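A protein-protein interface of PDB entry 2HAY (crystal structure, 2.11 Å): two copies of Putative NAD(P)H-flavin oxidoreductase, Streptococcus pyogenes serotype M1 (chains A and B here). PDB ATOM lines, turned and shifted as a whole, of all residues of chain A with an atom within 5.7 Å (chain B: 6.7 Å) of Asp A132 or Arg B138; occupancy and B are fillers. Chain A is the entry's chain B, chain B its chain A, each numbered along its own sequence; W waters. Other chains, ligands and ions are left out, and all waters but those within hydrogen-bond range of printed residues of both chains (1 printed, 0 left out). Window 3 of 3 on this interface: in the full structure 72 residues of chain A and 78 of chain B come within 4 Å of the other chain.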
ATOM      1  N   PHE A 126     -31.957  -1.773  21.276  1.00  0.00           N
ATOM      2  CA  PHE A 126     -30.600  -1.426  21.687  1.00  0.00           C
ATOM      3  C   PHE A 126     -30.207  -2.152  22.985  1.00  0.00           C
ATOM      4  O   PHE A 126     -29.128  -2.737  23.063  1.00  0.00           O
ATOM      5  CB  PHE A 126     -30.445   0.088  21.848  1.00  0.00           C
ATOM      6  CG  PHE A 126     -29.121   0.516  22.444  1.00  0.00           C
ATOM      7  CD1 PHE A 126     -29.067   1.137  23.699  1.00  0.00           C
ATOM      8  CD2 PHE A 126     -27.919   0.316  21.738  1.00  0.00           C
ATOM      9  CE1 PHE A 126     -27.824   1.554  24.244  1.00  0.00           C
ATOM     10  CE2 PHE A 126     -26.685   0.711  22.262  1.00  0.00           C
ATOM     11  CZ  PHE A 126     -26.623   1.331  23.505  1.00  0.00           C
ATOM     12  N   GLN A 127     -31.075  -2.130  23.993  1.00  0.00           N
ATOM     13  CA  GLN A 127     -30.771  -2.810  25.265  1.00  0.00           C
ATOM     14  C   GLN A 127     -30.953  -4.327  25.231  1.00  0.00           C
ATOM     15  O   GLN A 127     -30.251  -5.046  25.925  1.00  0.00           O
ATOM     16  CB  GLN A 127     -31.590  -2.213  26.409  1.00  0.00           C
ATOM     17  CG  GLN A 127     -31.215  -0.749  26.744  1.00  0.00           C
ATOM     18  CD  GLN A 127     -31.769  -0.303  28.086  1.00  0.00           C
ATOM     19  OE1 GLN A 127     -32.679  -0.928  28.627  1.00  0.00           O
ATOM     20  NE2 GLN A 127     -31.217   0.770  28.633  1.00  0.00           N
ATOM     21  N   LYS A 128     -31.894  -4.815  24.433  1.00  0.00           N
ATOM     22  CA  LYS A 128     -32.177  -6.244  24.378  1.00  0.00           C
ATOM     23  C   LYS A 128     -31.245  -6.981  23.413  1.00  0.00           C
ATOM     24  O   LYS A 128     -30.790  -8.083  23.717  1.00  0.00           O
ATOM     25  CB  LYS A 128     -33.632  -6.509  23.973  1.00  0.00           C
ATOM     26  CG  LYS A 128     -34.660  -6.114  25.000  1.00  0.00           C
ATOM     27  CD  LYS A 128     -36.050  -6.642  24.653  1.00  0.00           C
ATOM     28  CE  LYS A 128     -36.943  -6.528  25.895  1.00  0.00           C
ATOM     29  NZ  LYS A 128     -38.384  -6.497  25.547  1.00  0.00           N
ATOM     30  N   GLU A 129     -30.932  -6.347  22.283  1.00  0.00           N
ATOM     31  CA  GLU A 129     -30.232  -7.025  21.192  1.00  0.00           C
ATOM     32  C   GLU A 129     -28.801  -6.526  20.933  1.00  0.00           C
ATOM     33  O   GLU A 129     -27.882  -7.336  20.856  1.00  0.00           O
ATOM     34  CB  GLU A 129     -31.100  -7.013  19.926  1.00  0.00           C
ATOM     35  CG  GLU A 129     -32.413  -7.808  20.114  1.00  0.00           C
ATOM     36  CD  GLU A 129     -33.630  -7.110  19.534  1.00  0.00           C
ATOM     37  OE1 GLU A 129     -33.590  -6.778  18.323  1.00  0.00           O
ATOM     38  OE2 GLU A 129     -34.622  -6.903  20.295  1.00  0.00           O
ATOM     39  N   ASP A 130     -28.614  -5.210  20.832  1.00  0.00           N
ATOM     40  CA  ASP A 130     -27.280  -4.604  20.586  1.00  0.00           C
ATOM     41  C   ASP A 130     -26.318  -4.792  21.746  1.00  0.00           C
ATOM     42  O   ASP A 130     -25.194  -5.215  21.540  1.00  0.00           O
ATOM     43  CB  ASP A 130     -27.385  -3.121  20.225  1.00  0.00           C
ATOM     44  CG  ASP A 130     -28.215  -2.894  18.992  1.00  0.00           C
ATOM     45  OD1 ASP A 130     -28.363  -3.840  18.224  1.00  0.00           O
ATOM     46  OD2 ASP A 130     -28.735  -1.785  18.786  1.00  0.00           O
ATOM     47  N   MET A 131     -26.787  -4.509  22.963  1.00  0.00           N
ATOM     48  CA  MET A 131     -25.943  -4.547  24.172  1.00  0.00           C
ATOM     49  C   MET A 131     -26.273  -5.700  25.127  1.00  0.00           C
ATOM     50  O   MET A 131     -25.532  -5.934  26.083  1.00  0.00           O
ATOM     51  CB  MET A 131     -26.037  -3.220  24.931  1.00  0.00           C
ATOM     52  CG  MET A 131     -25.422  -2.024  24.195  1.00  0.00           C
ATOM     53  SD  MET A 131     -24.209  -0.990  25.337  1.00  0.00           S
ATOM     54  CE  MET A 131     -22.948  -2.451  25.392  1.00  0.00           C
ATOM     55  N   ASP A 132     -27.383  -6.403  24.870  1.00  0.00           N
ATOM     56  CA  ASP A 132     -27.787  -7.578  25.663  1.00  0.00           C
ATOM     57  C   ASP A 132     -27.800  -7.293  27.179  1.00  0.00           C
ATOM     58  O   ASP A 132     -27.071  -7.925  27.950  1.00  0.00           O
ATOM     59  CB  ASP A 132     -26.874  -8.775  25.316  1.00  0.00           C
ATOM     60  CG  ASP A 132     -27.350 -10.097  25.933  1.00  0.00           C
ATOM     61  OD1 ASP A 132     -28.577 -10.309  26.068  1.00  0.00           O
ATOM     62  OD2 ASP A 132     -26.478 -10.929  26.268  1.00  0.00           O
ATOM     63  N   MET A 133     -28.615  -6.323  27.607  1.00  0.00           N
ATOM     64  CA  MET A 133     -28.585  -5.869  28.993  1.00  0.00           C
ATOM     65  C   MET A 133     -29.953  -5.441  29.572  1.00  0.00           C
ATOM     66  O   MET A 133     -30.048  -5.178  30.743  1.00  0.00           O
ATOM     67  CB  MET A 133     -27.560  -4.726  29.159  1.00  0.00           C
ATOM     68  CG  MET A 133     -27.898  -3.492  28.327  1.00  0.00           C
ATOM     69  SD  MET A 133     -26.653  -2.010  28.626  1.00  0.00           S
ATOM     70  CE  MET A 133     -27.586  -0.652  27.666  1.00  0.00           C
ATOM     71  N   ALA A 134     -30.990  -5.357  28.749  1.00  0.00           N
ATOM     72  CA  ALA A 134     -32.309  -4.947  29.209  1.00  0.00           C
ATOM     73  C   ALA A 134     -32.722  -5.613  30.519  1.00  0.00           C
ATOM     74  O   ALA A 134     -33.362  -4.978  31.342  1.00  0.00           O
ATOM     75  CB  ALA A 134     -33.362  -5.241  28.141  1.00  0.00           C
ATOM     76  N   ASN A 136     -30.817  -7.240  32.859  1.00  0.00           N
ATOM     77  CA  ASN A 136     -29.616  -7.533  33.602  1.00  0.00           C
ATOM     78  C   ASN A 136     -29.158  -6.288  34.364  1.00  0.00           C
ATOM     79  O   ASN A 136     -28.323  -5.542  33.871  1.00  0.00           O
ATOM     80  CB  ASN A 136     -28.537  -7.971  32.602  1.00  0.00           C
ATOM     81  CG  ASN A 136     -27.276  -8.444  33.272  1.00  0.00           C
ATOM     82  OD1 ASN A 136     -26.971  -8.069  34.395  1.00  0.00           O
ATOM     83  ND2 ASN A 136     -26.531  -9.279  32.577  1.00  0.00           N
ATOM     84  N   ALA A 139     -25.443  -5.219  34.487  1.00  0.00           N
ATOM     85  CA  ALA A 139     -24.988  -4.737  33.175  1.00  0.00           C
ATOM     86  C   ALA A 139     -25.491  -3.312  32.906  1.00  0.00           C
ATOM     87  O   ALA A 139     -24.786  -2.487  32.364  1.00  0.00           O
ATOM     88  CB  ALA A 139     -25.411  -5.705  32.028  1.00  0.00           C
ATOM     89  N   MET B 133     -16.556  -8.945  40.654  1.00  0.00           N
ATOM     90  CA  MET B 133     -16.604  -9.182  39.199  1.00  0.00           C
ATOM     91  C   MET B 133     -15.720 -10.340  38.706  1.00  0.00           C
ATOM     92  O   MET B 133     -15.797 -10.706  37.532  1.00  0.00           O
ATOM     93  CB  MET B 133     -16.218  -7.906  38.446  1.00  0.00           C
ATOM     94  CG  MET B 133     -14.735  -7.621  38.469  1.00  0.00           C
ATOM     95  SD  MET B 133     -14.301  -5.940  37.660  1.00  0.00           S
ATOM     96  CE  MET B 133     -12.461  -5.782  38.151  1.00  0.00           C
ATOM     97  N   ASN B 136     -17.333 -13.275  36.809  1.00  0.00           N
ATOM     98  CA  ASN B 136     -18.351 -12.762  35.918  1.00  0.00           C
ATOM     99  C   ASN B 136     -17.634 -12.127  34.699  1.00  0.00           C
ATOM    100  O   ASN B 136     -17.278 -10.936  34.730  1.00  0.00           O
ATOM    101  CB  ASN B 136     -19.174 -11.734  36.724  1.00  0.00           C
ATOM    102  CG  ASN B 136     -20.367 -11.185  35.973  1.00  0.00           C
ATOM    103  OD1 ASN B 136     -20.434 -11.229  34.751  1.00  0.00           O
ATOM    104  ND2 ASN B 136     -21.319 -10.626  36.722  1.00  0.00           N
ATOM    105  N   PRO B 137     -17.402 -12.922  33.629  1.00  0.00           N
ATOM    106  CA  PRO B 137     -16.712 -12.453  32.416  1.00  0.00           C
ATOM    107  C   PRO B 137     -17.314 -11.202  31.759  1.00  0.00           C
ATOM    108  O   PRO B 137     -16.564 -10.362  31.316  1.00  0.00           O
ATOM    109  CB  PRO B 137     -16.796 -13.656  31.468  1.00  0.00           C
ATOM    110  CG  PRO B 137     -16.881 -14.845  32.385  1.00  0.00           C
ATOM    111  CD  PRO B 137     -17.777 -14.347  33.510  1.00  0.00           C
ATOM    112  N   ARG B 138     -18.639 -11.083  31.717  1.00  0.00           N
ATOM    113  CA  ARG B 138     -19.303  -9.868  31.224  1.00  0.00           C
ATOM    114  C   ARG B 138     -18.877  -8.634  32.064  1.00  0.00           C
ATOM    115  O   ARG B 138     -18.572  -7.575  31.497  1.00  0.00           O
ATOM    116  CB  ARG B 138     -20.839 -10.031  31.199  1.00  0.00           C
ATOM    117  CG  ARG B 138     -21.663  -8.723  31.117  1.00  0.00           C
ATOM    118  CD  ARG B 138     -21.615  -8.203  29.724  1.00  0.00           C
ATOM    119  NE  ARG B 138     -22.336  -6.952  29.459  1.00  0.00           N
ATOM    120  CZ  ARG B 138     -23.541  -6.874  28.888  1.00  0.00           C
ATOM    121  NH1 ARG B 138     -24.239  -7.970  28.633  1.00  0.00           N
ATOM    122  NH2 ARG B 138     -24.077  -5.693  28.625  1.00  0.00           N
ATOM    123  N   ALA B 139     -18.835  -8.786  33.389  1.00  0.00           N
ATOM    124  CA  ALA B 139     -18.408  -7.698  34.278  1.00  0.00           C
ATOM    125  C   ALA B 139     -16.917  -7.354  34.150  1.00  0.00           C
ATOM    126  O   ALA B 139     -16.562  -6.179  34.219  1.00  0.00           O
ATOM    127  CB  ALA B 139     -18.780  -7.984  35.723  1.00  0.00           C
ATOM    128  N   LEU B 140     -16.065  -8.368  33.975  1.00  0.00           N
ATOM    129  CA  LEU B 140     -14.657  -8.159  33.631  1.00  0.00           C
ATOM    130  C   LEU B 140     -14.480  -7.446  32.301  1.00  0.00           C
ATOM    131  O   LEU B 140     -13.634  -6.555  32.190  1.00  0.00           O
ATOM    132  CB  LEU B 140     -13.871  -9.477  33.610  1.00  0.00           C
ATOM    133  CG  LEU B 140     -13.448 -10.051  34.962  1.00  0.00           C
ATOM    134  CD1 LEU B 140     -12.779 -11.390  34.739  1.00  0.00           C
ATOM    135  CD2 LEU B 140     -12.518  -9.054  35.703  1.00  0.00           C
ATOM    136  N   PHE B 141     -15.260  -7.840  31.288  1.00  0.00           N
ATOM    137  CA  PHE B 141     -15.240  -7.111  30.025  1.00  0.00           C
ATOM    138  C   PHE B 141     -15.744  -5.687  30.194  1.00  0.00           C
ATOM    139  O   PHE B 141     -15.160  -4.742  29.659  1.00  0.00           O
ATOM    140  CB  PHE B 141     -16.010  -7.806  28.891  1.00  0.00           C
ATOM    141  CG  PHE B 141     -16.043  -6.972  27.629  1.00  0.00           C
ATOM    142  CD1 PHE B 141     -14.928  -6.925  26.780  1.00  0.00           C
ATOM    143  CD2 PHE B 141     -17.134  -6.137  27.361  1.00  0.00           C
ATOM    144  CE1 PHE B 141     -14.919  -6.106  25.654  1.00  0.00           C
ATOM    145  CE2 PHE B 141     -17.152  -5.300  26.242  1.00  0.00           C
ATOM    146  CZ  PHE B 141     -16.045  -5.281  25.384  1.00  0.00           C
ATOM    147  N   ASP B 142     -16.852  -5.515  30.908  1.00  0.00           N
ATOM    148  CA  ASP B 142     -17.408  -4.170  31.119  1.00  0.00           C
ATOM    149  C   ASP B 142     -16.432  -3.254  31.892  1.00  0.00           C
ATOM    150  O   ASP B 142     -16.415  -2.059  31.653  1.00  0.00           O
ATOM    151  CB  ASP B 142     -18.750  -4.273  31.819  1.00  0.00           C
ATOM    152  CG  ASP B 142     -19.900  -4.564  30.843  1.00  0.00           C
ATOM    153  OD1 ASP B 142     -19.716  -4.358  29.605  1.00  0.00           O
ATOM    154  OD2 ASP B 142     -20.990  -4.980  31.319  1.00  0.00           O
ATOM    155  N   TRP B 143     -15.610  -3.831  32.786  1.00  0.00           N
ATOM    156  CA  TRP B 143     -14.548  -3.111  33.484  1.00  0.00           C
ATOM    157  C   TRP B 143     -13.410  -2.596  32.581  1.00  0.00           C
ATOM    158  O   TRP B 143     -13.003  -1.434  32.689  1.00  0.00           O
ATOM    159  CB  TRP B 143     -13.967  -3.995  34.596  1.00  0.00           C
ATOM    160  CG  TRP B 143     -12.754  -3.399  35.313  1.00  0.00           C
ATOM    161  CD1 TRP B 143     -12.717  -2.234  36.044  1.00  0.00           C
ATOM    162  CD2 TRP B 143     -11.418  -3.934  35.347  1.00  0.00           C
ATOM    163  NE1 TRP B 143     -11.437  -2.030  36.567  1.00  0.00           N
ATOM    164  CE2 TRP B 143     -10.621  -3.044  36.137  1.00  0.00           C
ATOM    165  CE3 TRP B 143     -10.815  -5.084  34.798  1.00  0.00           C
ATOM    166  CZ2 TRP B 143      -9.251  -3.269  36.394  1.00  0.00           C
ATOM    167  CZ3 TRP B 143      -9.430  -5.311  35.045  1.00  0.00           C
ATOM    168  CH2 TRP B 143      -8.669  -4.399  35.837  1.00  0.00           C
HETATM  169  O   HOH W   1     -22.856  -3.315  30.570  1.00  0.00           O
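The guanidinium group (NH2) of Arg B138 sits at hydrogen-bond distance from the backbone carbonyl oxygen (O) of Met A131 (2.9 Å).
The guanidinium group (NH1) of Arg B138 sits at hydrogen-bond distance from the backbone carbonyl oxygen (O) of Asp A132.
The backbone NH of Met A131 lies within hydrogen-bond range of the backbone carbonyl oxygen of Phe A126, 2.9 Å away.
The backbone carbonyl oxygen of Gln A127 is in hydrogen-bond range of the backbone NH of Asp A132 (3.3 Å).
The backbone carbonyl oxygen (O) of Gln A127 is in hydrogen-bond range of the backbone NH (N) of Met A133.
The side-chain carboxylate (OD2) of Asp B142 lies within salt-bridge range of the guanidinium group (NE) of Arg B138, 3.0 Å away.
The backbone NH of Ala A139 lies within hydrogen-bond range of the side-chain amide oxygen of Asn A136 (3.2 Å).
NH2 of Arg B138 touches CB of Met A133, 3.7 Å away.
Ala A139 touches Arg B138 (CB to NH2, 3.7 Å).
Of chain B, only Arg B138 comes within 4 Å of Asp A132.
Arg B138 touches just these residues of chain A: Met A131, Asp A132, Met A133 and Ala A139.
Of the printed residues of chain B, Met A133 touches Arg B138 (3.7 Å).
Of the printed residues of chain B, Met A131 touches Arg B138 (2.9 Å).
Printed residues of chain B within 4 Å of Ala A139: Arg B138.
Phe A126 touches none of the printed residues of chain B.
The nearest printed residue of chain B that does not touch Asp A132 is Asp B142 (7.5 Å).
The nearest residue of chain A that does not touch Arg B138 is Asn A136 (4.7 Å).
Of the 9 printed residues of chain B, 1 touches a printed residue of chain A.
Hydrophobic or aromatic side chains of chain A within 4 Å of the printed part of chain B: Met A133 and Ala A139.
Among the printed residues, 4 pairs touch across the chains.
Positions printed for both chains: 133, 136 and 139.
Of the 4 pairs that touch across the chains among the printed residues, none has its exchanged pair printed and touching as well.
Water W1 lies within hydrogen-bond range of the side-chain carboxylate of Asp B142, the backbone carbonyl oxygen of Ala A139 and the guanidinium group of Arg B138.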
